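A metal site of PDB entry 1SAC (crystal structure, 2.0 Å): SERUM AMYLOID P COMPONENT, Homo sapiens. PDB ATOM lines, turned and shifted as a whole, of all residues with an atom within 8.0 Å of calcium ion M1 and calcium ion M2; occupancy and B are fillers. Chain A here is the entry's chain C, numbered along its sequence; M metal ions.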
ATOM      1  N   SER A  48     -18.768  18.118 -15.649  1.00  0.00           N
ATOM      2  CA  SER A  48     -18.889  19.197 -14.659  1.00  0.00           C
ATOM      3  C   SER A  48     -17.590  19.986 -14.571  1.00  0.00           C
ATOM      4  O   SER A  48     -16.535  19.387 -14.394  1.00  0.00           O
ATOM      5  CB  SER A  48     -19.230  18.603 -13.293  1.00  0.00           C
ATOM      6  OG  SER A  48     -19.202  19.595 -12.276  1.00  0.00           O
ATOM      7  N   SER A  51     -18.597  22.457  -9.220  1.00  0.00           N
ATOM      8  CA  SER A  51     -19.693  21.833  -8.462  1.00  0.00           C
ATOM      9  C   SER A  51     -19.697  22.393  -7.027  1.00  0.00           C
ATOM     10  O   SER A  51     -18.809  22.068  -6.229  1.00  0.00           O
ATOM     11  CB  SER A  51     -19.516  20.325  -8.466  1.00  0.00           C
ATOM     12  OG  SER A  51     -20.501  19.707  -7.641  1.00  0.00           O
ATOM     13  N   TYR A  52     -20.731  23.196  -6.780  1.00  0.00           N
ATOM     14  CA  TYR A  52     -20.976  23.939  -5.513  1.00  0.00           C
ATOM     15  C   TYR A  52     -22.348  23.472  -4.948  1.00  0.00           C
ATOM     16  O   TYR A  52     -23.404  23.888  -5.441  1.00  0.00           O
ATOM     17  CB  TYR A  52     -20.970  25.437  -5.897  1.00  0.00           C
ATOM     18  CG  TYR A  52     -21.245  26.471  -4.776  1.00  0.00           C
ATOM     19  CD1 TYR A  52     -22.409  26.416  -4.005  1.00  0.00           C
ATOM     20  CD2 TYR A  52     -20.317  27.516  -4.548  1.00  0.00           C
ATOM     21  CE1 TYR A  52     -22.657  27.392  -3.016  1.00  0.00           C
ATOM     22  CE2 TYR A  52     -20.564  28.493  -3.581  1.00  0.00           C
ATOM     23  CZ  TYR A  52     -21.742  28.437  -2.815  1.00  0.00           C
ATOM     24  OH  TYR A  52     -21.987  29.386  -1.873  1.00  0.00           O
ATOM     25  N   ASN A  53     -22.277  22.596  -3.951  1.00  0.00           N
ATOM     26  CA  ASN A  53     -23.475  22.007  -3.284  1.00  0.00           C
ATOM     27  C   ASN A  53     -23.516  22.447  -1.812  1.00  0.00           C
ATOM     28  O   ASN A  53     -22.475  22.691  -1.187  1.00  0.00           O
ATOM     29  CB  ASN A  53     -23.398  20.474  -3.302  1.00  0.00           C
ATOM     30  CG  ASN A  53     -24.107  19.827  -4.486  1.00  0.00           C
ATOM     31  OD1 ASN A  53     -24.157  20.418  -5.569  1.00  0.00           O
ATOM     32  ND2 ASN A  53     -24.651  18.626  -4.364  1.00  0.00           N
ATOM     33  N   ARG A  57     -28.993  20.405  -0.601  1.00  0.00           N
ATOM     34  CA  ARG A  57     -29.322  21.088  -1.851  1.00  0.00           C
ATOM     35  C   ARG A  57     -28.324  20.736  -2.939  1.00  0.00           C
ATOM     36  O   ARG A  57     -27.148  21.101  -2.858  1.00  0.00           O
ATOM     37  CB  ARG A  57     -29.337  22.599  -1.635  1.00  0.00           C
ATOM     38  CG  ARG A  57     -30.656  22.964  -0.939  1.00  0.00           C
ATOM     39  CD  ARG A  57     -30.525  24.378  -0.364  1.00  0.00           C
ATOM     40  NE  ARG A  57     -31.658  25.229  -0.781  1.00  0.00           N
ATOM     41  CZ  ARG A  57     -31.757  26.497  -0.335  1.00  0.00           C
ATOM     42  NH1 ARG A  57     -30.897  26.957   0.565  1.00  0.00           N
ATOM     43  NH2 ARG A  57     -32.717  27.304  -0.789  1.00  0.00           N
ATOM     44  N   ASP A  58     -28.778  20.030  -3.950  1.00  0.00           N
ATOM     45  CA  ASP A  58     -27.975  19.651  -5.122  1.00  0.00           C
ATOM     46  C   ASP A  58     -27.891  20.801  -6.111  1.00  0.00           C
ATOM     47  O   ASP A  58     -28.866  21.540  -6.242  1.00  0.00           O
ATOM     48  CB  ASP A  58     -28.610  18.433  -5.807  1.00  0.00           C
ATOM     49  CG  ASP A  58     -27.601  17.797  -6.776  1.00  0.00           C
ATOM     50  OD1 ASP A  58     -26.412  17.819  -6.463  1.00  0.00           O
ATOM     51  OD2 ASP A  58     -28.063  17.299  -7.812  1.00  0.00           O
ATOM     52  N   ASN A  59     -26.776  20.967  -6.792  1.00  0.00           N
ATOM     53  CA  ASN A  59     -26.664  21.890  -7.932  1.00  0.00           C
ATOM     54  C   ASN A  59     -27.054  23.311  -7.501  1.00  0.00           C
ATOM     55  O   ASN A  59     -27.757  24.024  -8.215  1.00  0.00           O
ATOM     56  CB  ASN A  59     -27.587  21.438  -9.071  1.00  0.00           C
ATOM     57  CG  ASN A  59     -27.075  20.197  -9.792  1.00  0.00           C
ATOM     58  OD1 ASN A  59     -25.976  19.726  -9.493  1.00  0.00           O
ATOM     59  ND2 ASN A  59     -27.788  19.634 -10.742  1.00  0.00           N
ATOM     60  N   GLU A  60     -26.620  23.649  -6.305  1.00  0.00           N
ATOM     61  CA  GLU A  60     -26.811  25.024  -5.797  1.00  0.00           C
ATOM     62  C   GLU A  60     -26.110  26.020  -6.697  1.00  0.00           C
ATOM     63  O   GLU A  60     -26.648  27.046  -7.091  1.00  0.00           O
ATOM     64  CB  GLU A  60     -26.328  25.124  -4.367  1.00  0.00           C
ATOM     65  CG  GLU A  60     -26.688  26.468  -3.751  1.00  0.00           C
ATOM     66  CD  GLU A  60     -28.187  26.677  -3.622  1.00  0.00           C
ATOM     67  OE1 GLU A  60     -29.001  25.782  -3.833  1.00  0.00           O
ATOM     68  OE2 GLU A  60     -28.605  27.802  -3.290  1.00  0.00           O
ATOM     69  N   LEU A  62     -23.586  25.280 -10.280  1.00  0.00           N
ATOM     70  CA  LEU A  62     -22.925  24.232 -11.101  1.00  0.00           C
ATOM     71  C   LEU A  62     -22.593  24.784 -12.479  1.00  0.00           C
ATOM     72  O   LEU A  62     -23.501  25.239 -13.166  1.00  0.00           O
ATOM     73  CB  LEU A  62     -23.771  22.988 -11.181  1.00  0.00           C
ATOM     74  CG  LEU A  62     -23.375  21.876 -12.118  1.00  0.00           C
ATOM     75  CD1 LEU A  62     -22.001  21.297 -11.847  1.00  0.00           C
ATOM     76  CD2 LEU A  62     -24.394  20.737 -12.122  1.00  0.00           C
ATOM     77  N   TYR A  64     -21.442  23.553 -16.076  1.00  0.00           N
ATOM     78  CA  TYR A  64     -21.539  22.228 -16.726  1.00  0.00           C
ATOM     79  C   TYR A  64     -21.268  22.400 -18.217  1.00  0.00           C
ATOM     80  O   TYR A  64     -21.808  23.335 -18.827  1.00  0.00           O
ATOM     81  CB  TYR A  64     -22.893  21.616 -16.486  1.00  0.00           C
ATOM     82  CG  TYR A  64     -23.006  20.109 -16.645  1.00  0.00           C
ATOM     83  CD1 TYR A  64     -22.644  19.252 -15.601  1.00  0.00           C
ATOM     84  CD2 TYR A  64     -23.489  19.573 -17.845  1.00  0.00           C
ATOM     85  CE1 TYR A  64     -22.757  17.868 -15.761  1.00  0.00           C
ATOM     86  CE2 TYR A  64     -23.600  18.192 -17.991  1.00  0.00           C
ATOM     87  CZ  TYR A  64     -23.235  17.338 -16.956  1.00  0.00           C
ATOM     88  OH  TYR A  64     -23.347  15.971 -17.097  1.00  0.00           O
ATOM     89  N   TYR A  74     -26.185  26.301 -13.519  1.00  0.00           N
ATOM     90  CA  TYR A  74     -27.297  25.996 -12.621  1.00  0.00           C
ATOM     91  C   TYR A  74     -27.213  26.880 -11.388  1.00  0.00           C
ATOM     92  O   TYR A  74     -26.157  26.987 -10.762  1.00  0.00           O
ATOM     93  CB  TYR A  74     -27.256  24.566 -12.061  1.00  0.00           C
ATOM     94  CG  TYR A  74     -27.409  23.426 -13.065  1.00  0.00           C
ATOM     95  CD1 TYR A  74     -26.480  23.286 -14.093  1.00  0.00           C
ATOM     96  CD2 TYR A  74     -28.474  22.509 -12.950  1.00  0.00           C
ATOM     97  CE1 TYR A  74     -26.581  22.223 -14.996  1.00  0.00           C
ATOM     98  CE2 TYR A  74     -28.575  21.445 -13.853  1.00  0.00           C
ATOM     99  CZ  TYR A  74     -27.635  21.301 -14.867  1.00  0.00           C
ATOM    100  OH  TYR A  74     -27.722  20.253 -15.747  1.00  0.00           O
ATOM    101  N   ARG A  77     -30.682  24.631  -8.621  1.00  0.00           N
ATOM    102  CA  ARG A  77     -31.289  23.540  -9.400  1.00  0.00           C
ATOM    103  C   ARG A  77     -31.982  24.057 -10.664  1.00  0.00           C
ATOM    104  O   ARG A  77     -32.494  23.264 -11.481  1.00  0.00           O
ATOM    105  CB  ARG A  77     -32.316  22.795  -8.543  1.00  0.00           C
ATOM    106  CG  ARG A  77     -31.696  21.673  -7.720  1.00  0.00           C
ATOM    107  CD  ARG A  77     -32.417  21.405  -6.394  1.00  0.00           C
ATOM    108  NE  ARG A  77     -32.621  22.606  -5.588  1.00  0.00           N
ATOM    109  CZ  ARG A  77     -31.633  23.376  -5.092  1.00  0.00           C
ATOM    110  NH1 ARG A  77     -30.349  23.070  -5.310  1.00  0.00           N
ATOM    111  NH2 ARG A  77     -31.836  24.471  -4.346  1.00  0.00           N
ATOM    112  N   GLN A 135     -15.051  16.246 -10.120  1.00  0.00           N
ATOM    113  CA  GLN A 135     -16.272  15.407 -10.051  1.00  0.00           C
ATOM    114  C   GLN A 135     -17.501  16.305  -9.868  1.00  0.00           C
ATOM    115  O   GLN A 135     -17.379  17.496  -9.548  1.00  0.00           O
ATOM    116  CB  GLN A 135     -16.230  14.433  -8.877  1.00  0.00           C
ATOM    117  CG  GLN A 135     -15.059  13.449  -8.923  1.00  0.00           C
ATOM    118  CD  GLN A 135     -15.224  12.328  -9.958  1.00  0.00           C
ATOM    119  OE1 GLN A 135     -16.345  11.969 -10.305  1.00  0.00           O
ATOM    120  NE2 GLN A 135     -14.156  11.755 -10.482  1.00  0.00           N
ATOM    121  N   GLU A 136     -18.651  15.694 -10.074  1.00  0.00           N
ATOM    122  CA  GLU A 136     -19.945  16.361  -9.916  1.00  0.00           C
ATOM    123  C   GLU A 136     -20.660  15.762  -8.703  1.00  0.00           C
ATOM    124  O   GLU A 136     -20.963  14.569  -8.662  1.00  0.00           O
ATOM    125  CB  GLU A 136     -20.772  16.164 -11.194  1.00  0.00           C
ATOM    126  CG  GLU A 136     -21.799  17.260 -11.414  1.00  0.00           C
ATOM    127  CD  GLU A 136     -23.013  17.112 -10.507  1.00  0.00           C
ATOM    128  OE1 GLU A 136     -23.548  15.953 -10.350  1.00  0.00           O
ATOM    129  OE2 GLU A 136     -23.494  18.144  -9.904  1.00  0.00           O
ATOM    130  N   GLN A 137     -20.924  16.610  -7.709  1.00  0.00           N
ATOM    131  CA  GLN A 137     -21.574  16.180  -6.452  1.00  0.00           C
ATOM    132  C   GLN A 137     -23.081  15.981  -6.616  1.00  0.00           C
ATOM    133  O   GLN A 137     -23.753  16.732  -7.337  1.00  0.00           O
ATOM    134  CB  GLN A 137     -21.448  17.255  -5.373  1.00  0.00           C
ATOM    135  CG  GLN A 137     -20.023  17.616  -4.992  1.00  0.00           C
ATOM    136  CD  GLN A 137     -19.976  18.769  -3.987  1.00  0.00           C
ATOM    137  OE1 GLN A 137     -20.101  18.541  -2.781  1.00  0.00           O
ATOM    138  NE2 GLN A 137     -19.824  20.007  -4.412  1.00  0.00           N
ATOM    139  N   ASP A 138     -23.576  14.970  -5.926  1.00  0.00           N
ATOM    140  CA  ASP A 138     -25.012  14.652  -5.897  1.00  0.00           C
ATOM    141  C   ASP A 138     -25.488  14.593  -4.442  1.00  0.00           C
ATOM    142  O   ASP A 138     -26.690  14.624  -4.156  1.00  0.00           O
ATOM    143  CB  ASP A 138     -25.300  13.317  -6.576  1.00  0.00           C
ATOM    144  CG  ASP A 138     -25.731  13.481  -8.029  1.00  0.00           C
ATOM    145  OD1 ASP A 138     -25.797  14.663  -8.537  1.00  0.00           O
ATOM    146  OD2 ASP A 138     -26.013  12.447  -8.731  1.00  0.00           O
ATOM    147  N   SER A 139     -24.467  14.842  -3.625  1.00  0.00           N
ATOM    148  CA  SER A 139     -24.671  15.043  -2.195  1.00  0.00           C
ATOM    149  C   SER A 139     -23.728  16.132  -1.687  1.00  0.00           C
ATOM    150  O   SER A 139     -23.055  16.799  -2.467  1.00  0.00           O
ATOM    151  CB  SER A 139     -24.456  13.769  -1.419  1.00  0.00           C
ATOM    152  OG  SER A 139     -23.061  13.404  -1.448  1.00  0.00           O
ATOM    153  N   GLY A 142     -20.200  14.593  -2.071  1.00  0.00           N
ATOM    154  CA  GLY A 142     -20.050  13.232  -2.610  1.00  0.00           C
ATOM    155  C   GLY A 142     -21.102  12.856  -3.624  1.00  0.00           C
ATOM    156  O   GLY A 142     -21.627  13.733  -4.314  1.00  0.00           O
ATOM    157  N   LYS A 143     -21.393  11.572  -3.735  1.00  0.00           N
ATOM    158  CA  LYS A 143     -22.287  10.997  -4.746  1.00  0.00           C
ATOM    159  C   LYS A 143     -21.858  11.432  -6.140  1.00  0.00           C
ATOM    160  O   LYS A 143     -22.622  12.057  -6.871  1.00  0.00           O
ATOM    161  CB  LYS A 143     -23.718  11.409  -4.500  1.00  0.00           C
ATOM    162  CG  LYS A 143     -24.453  10.495  -3.530  1.00  0.00           C
ATOM    163  CD  LYS A 143     -25.917  10.691  -3.858  1.00  0.00           C
ATOM    164  CE  LYS A 143     -27.205  11.464  -4.101  1.00  0.00           C
ATOM    165  NZ  LYS A 143     -27.878  12.231  -3.041  1.00  0.00           N
ATOM    166  N   PHE A 144     -20.630  11.076  -6.449  1.00  0.00           N
ATOM    167  CA  PHE A 144     -19.954  11.383  -7.716  1.00  0.00           C
ATOM    168  C   PHE A 144     -20.472  10.511  -8.838  1.00  0.00           C
ATOM    169  O   PHE A 144     -21.049   9.440  -8.611  1.00  0.00           O
ATOM    170  CB  PHE A 144     -18.448  11.240  -7.581  1.00  0.00           C
ATOM    171  CG  PHE A 144     -17.864  12.097  -6.452  1.00  0.00           C
ATOM    172  CD1 PHE A 144     -18.411  13.333  -6.141  1.00  0.00           C
ATOM    173  CD2 PHE A 144     -16.775  11.638  -5.723  1.00  0.00           C
ATOM    174  CE1 PHE A 144     -17.872  14.108  -5.113  1.00  0.00           C
ATOM    175  CE2 PHE A 144     -16.228  12.406  -4.695  1.00  0.00           C
ATOM    176  CZ  PHE A 144     -16.780  13.653  -4.392  1.00  0.00           C
ATOM    177  N   ASP A 145     -20.304  10.975 -10.060  1.00  0.00           N
ATOM    178  CA  ASP A 145     -20.768  10.245 -11.248  1.00  0.00           C
ATOM    179  C   ASP A 145     -19.675  10.191 -12.293  1.00  0.00           C
ATOM    180  O   ASP A 145     -19.187  11.192 -12.805  1.00  0.00           O
ATOM    181  CB  ASP A 145     -22.012  10.905 -11.828  1.00  0.00           C
ATOM    182  CG  ASP A 145     -22.649  10.079 -12.939  1.00  0.00           C
ATOM    183  OD1 ASP A 145     -21.960   9.341 -13.656  1.00  0.00           O
ATOM    184  OD2 ASP A 145     -23.865  10.193 -13.119  1.00  0.00           O
ATOM    185  N   ARG A 146     -19.239   8.993 -12.629  1.00  0.00           N
ATOM    186  CA  ARG A 146     -18.108   8.764 -13.529  1.00  0.00           C
ATOM    187  C   ARG A 146     -18.293   9.479 -14.862  1.00  0.00           C
ATOM    188  O   ARG A 146     -17.312   9.933 -15.451  1.00  0.00           O
ATOM    189  CB  ARG A 146     -18.012   7.242 -13.802  1.00  0.00           C
ATOM    190  CG  ARG A 146     -16.648   6.896 -14.392  1.00  0.00           C
ATOM    191  CD  ARG A 146     -16.840   5.389 -14.602  1.00  0.00           C
ATOM    192  NE  ARG A 146     -15.551   4.701 -14.807  1.00  0.00           N
ATOM    193  CZ  ARG A 146     -14.430   4.559 -14.049  1.00  0.00           C
ATOM    194  NH1 ARG A 146     -14.553   4.671 -12.733  1.00  0.00           N
ATOM    195  NH2 ARG A 146     -13.285   4.294 -14.660  1.00  0.00           N
ATOM    196  N   SER A 147     -19.516   9.590 -15.347  1.00  0.00           N
ATOM    197  CA  SER A 147     -19.754  10.134 -16.696  1.00  0.00           C
ATOM    198  C   SER A 147     -19.973  11.639 -16.662  1.00  0.00           C
ATOM    199  O   SER A 147     -20.225  12.240 -17.712  1.00  0.00           O
ATOM    200  CB  SER A 147     -20.936   9.462 -17.360  1.00  0.00           C
ATOM    201  OG  SER A 147     -22.081   9.552 -16.503  1.00  0.00           O
ATOM    202  N   GLN A 148     -19.808  12.234 -15.519  1.00  0.00           N
ATOM    203  CA  GLN A 148     -19.807  13.702 -15.443  1.00  0.00           C
ATOM    204  C   GLN A 148     -18.452  14.195 -14.936  1.00  0.00           C
ATOM    205  O   GLN A 148     -18.247  15.408 -14.738  1.00  0.00           O
ATOM    206  CB  GLN A 148     -20.901  14.176 -14.487  1.00  0.00           C
ATOM    207  CG  GLN A 148     -22.289  13.673 -14.884  1.00  0.00           C
ATOM    208  CD  GLN A 148     -23.389  14.140 -13.932  1.00  0.00           C
ATOM    209  OE1 GLN A 148     -23.317  13.897 -12.729  1.00  0.00           O
ATOM    210  NE2 GLN A 148     -24.424  14.813 -14.405  1.00  0.00           N
HETATM  211 CA    CA M   1     -24.695  13.801 -10.699  1.00  0.00          CA
HETATM  212 CA    CA M   2     -25.629  17.157  -8.966  1.00  0.00          CA
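The backbone carbonyl oxygen (O) of Gln 148 is in hydrogen-bond range of the backbone NH (N) of Ser 48 (2.9 Å). The side-chain amide oxygen of Gln 137 sits close to the backbone carbonyl oxygen of Ser 139, at 3.4 Å. O of Ser 51 lies within hydrogen-bond range of NE2 of Gln 137. The backbone carbonyl oxygen (O) of Asp 138 is in hydrogen-bond range of the side-chain amino group (NZ) of Lys 143. O of Asn 59 sits at hydrogen-bond distance from N of Arg 77, at 3.0 Å. The side-chain carboxylate of Asp 58 sits close to the side-chain amide nitrogen of Asn 53, 2.9 Å away. NE2 of Gln 148 sits at hydrogen-bond distance from OH of Tyr 64. The backbone NH (N) of Asn 59 is in hydrogen-bond range of the side-chain amide oxygen (OD1) of Asn 53, 2.9 Å away.
Of the 24 residues printed, 5 come within 4 Å of calcium ion M2.
The side-chain amide oxygen (OE1) of Gln 148 is bound to calcium ion M1 (2.5 Å). The side-chain carboxylate (OE1) of Glu 136 is bound to calcium ion M1, at 2.5 Å. The side-chain carboxylate (OD1) of Asp 138 binds calcium ion M1 (2.6 Å). The side-chain carboxylate (OD2) of Asp 138 binds calcium ion M1 (2.7 Å).
Calcium ion M2 is bound by O of Gln 137 (2.5 Å), OE2 of Glu 136 (2.5 Å), OD1 of Asp 138 (2.5 Å), OD1 of Asn 59 (2.6 Å), OD2 of Asp 58 (2.7 Å), OD1 of Asp 58 (2.7 Å) and OE1 of Glu 136 (2.8 Å).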
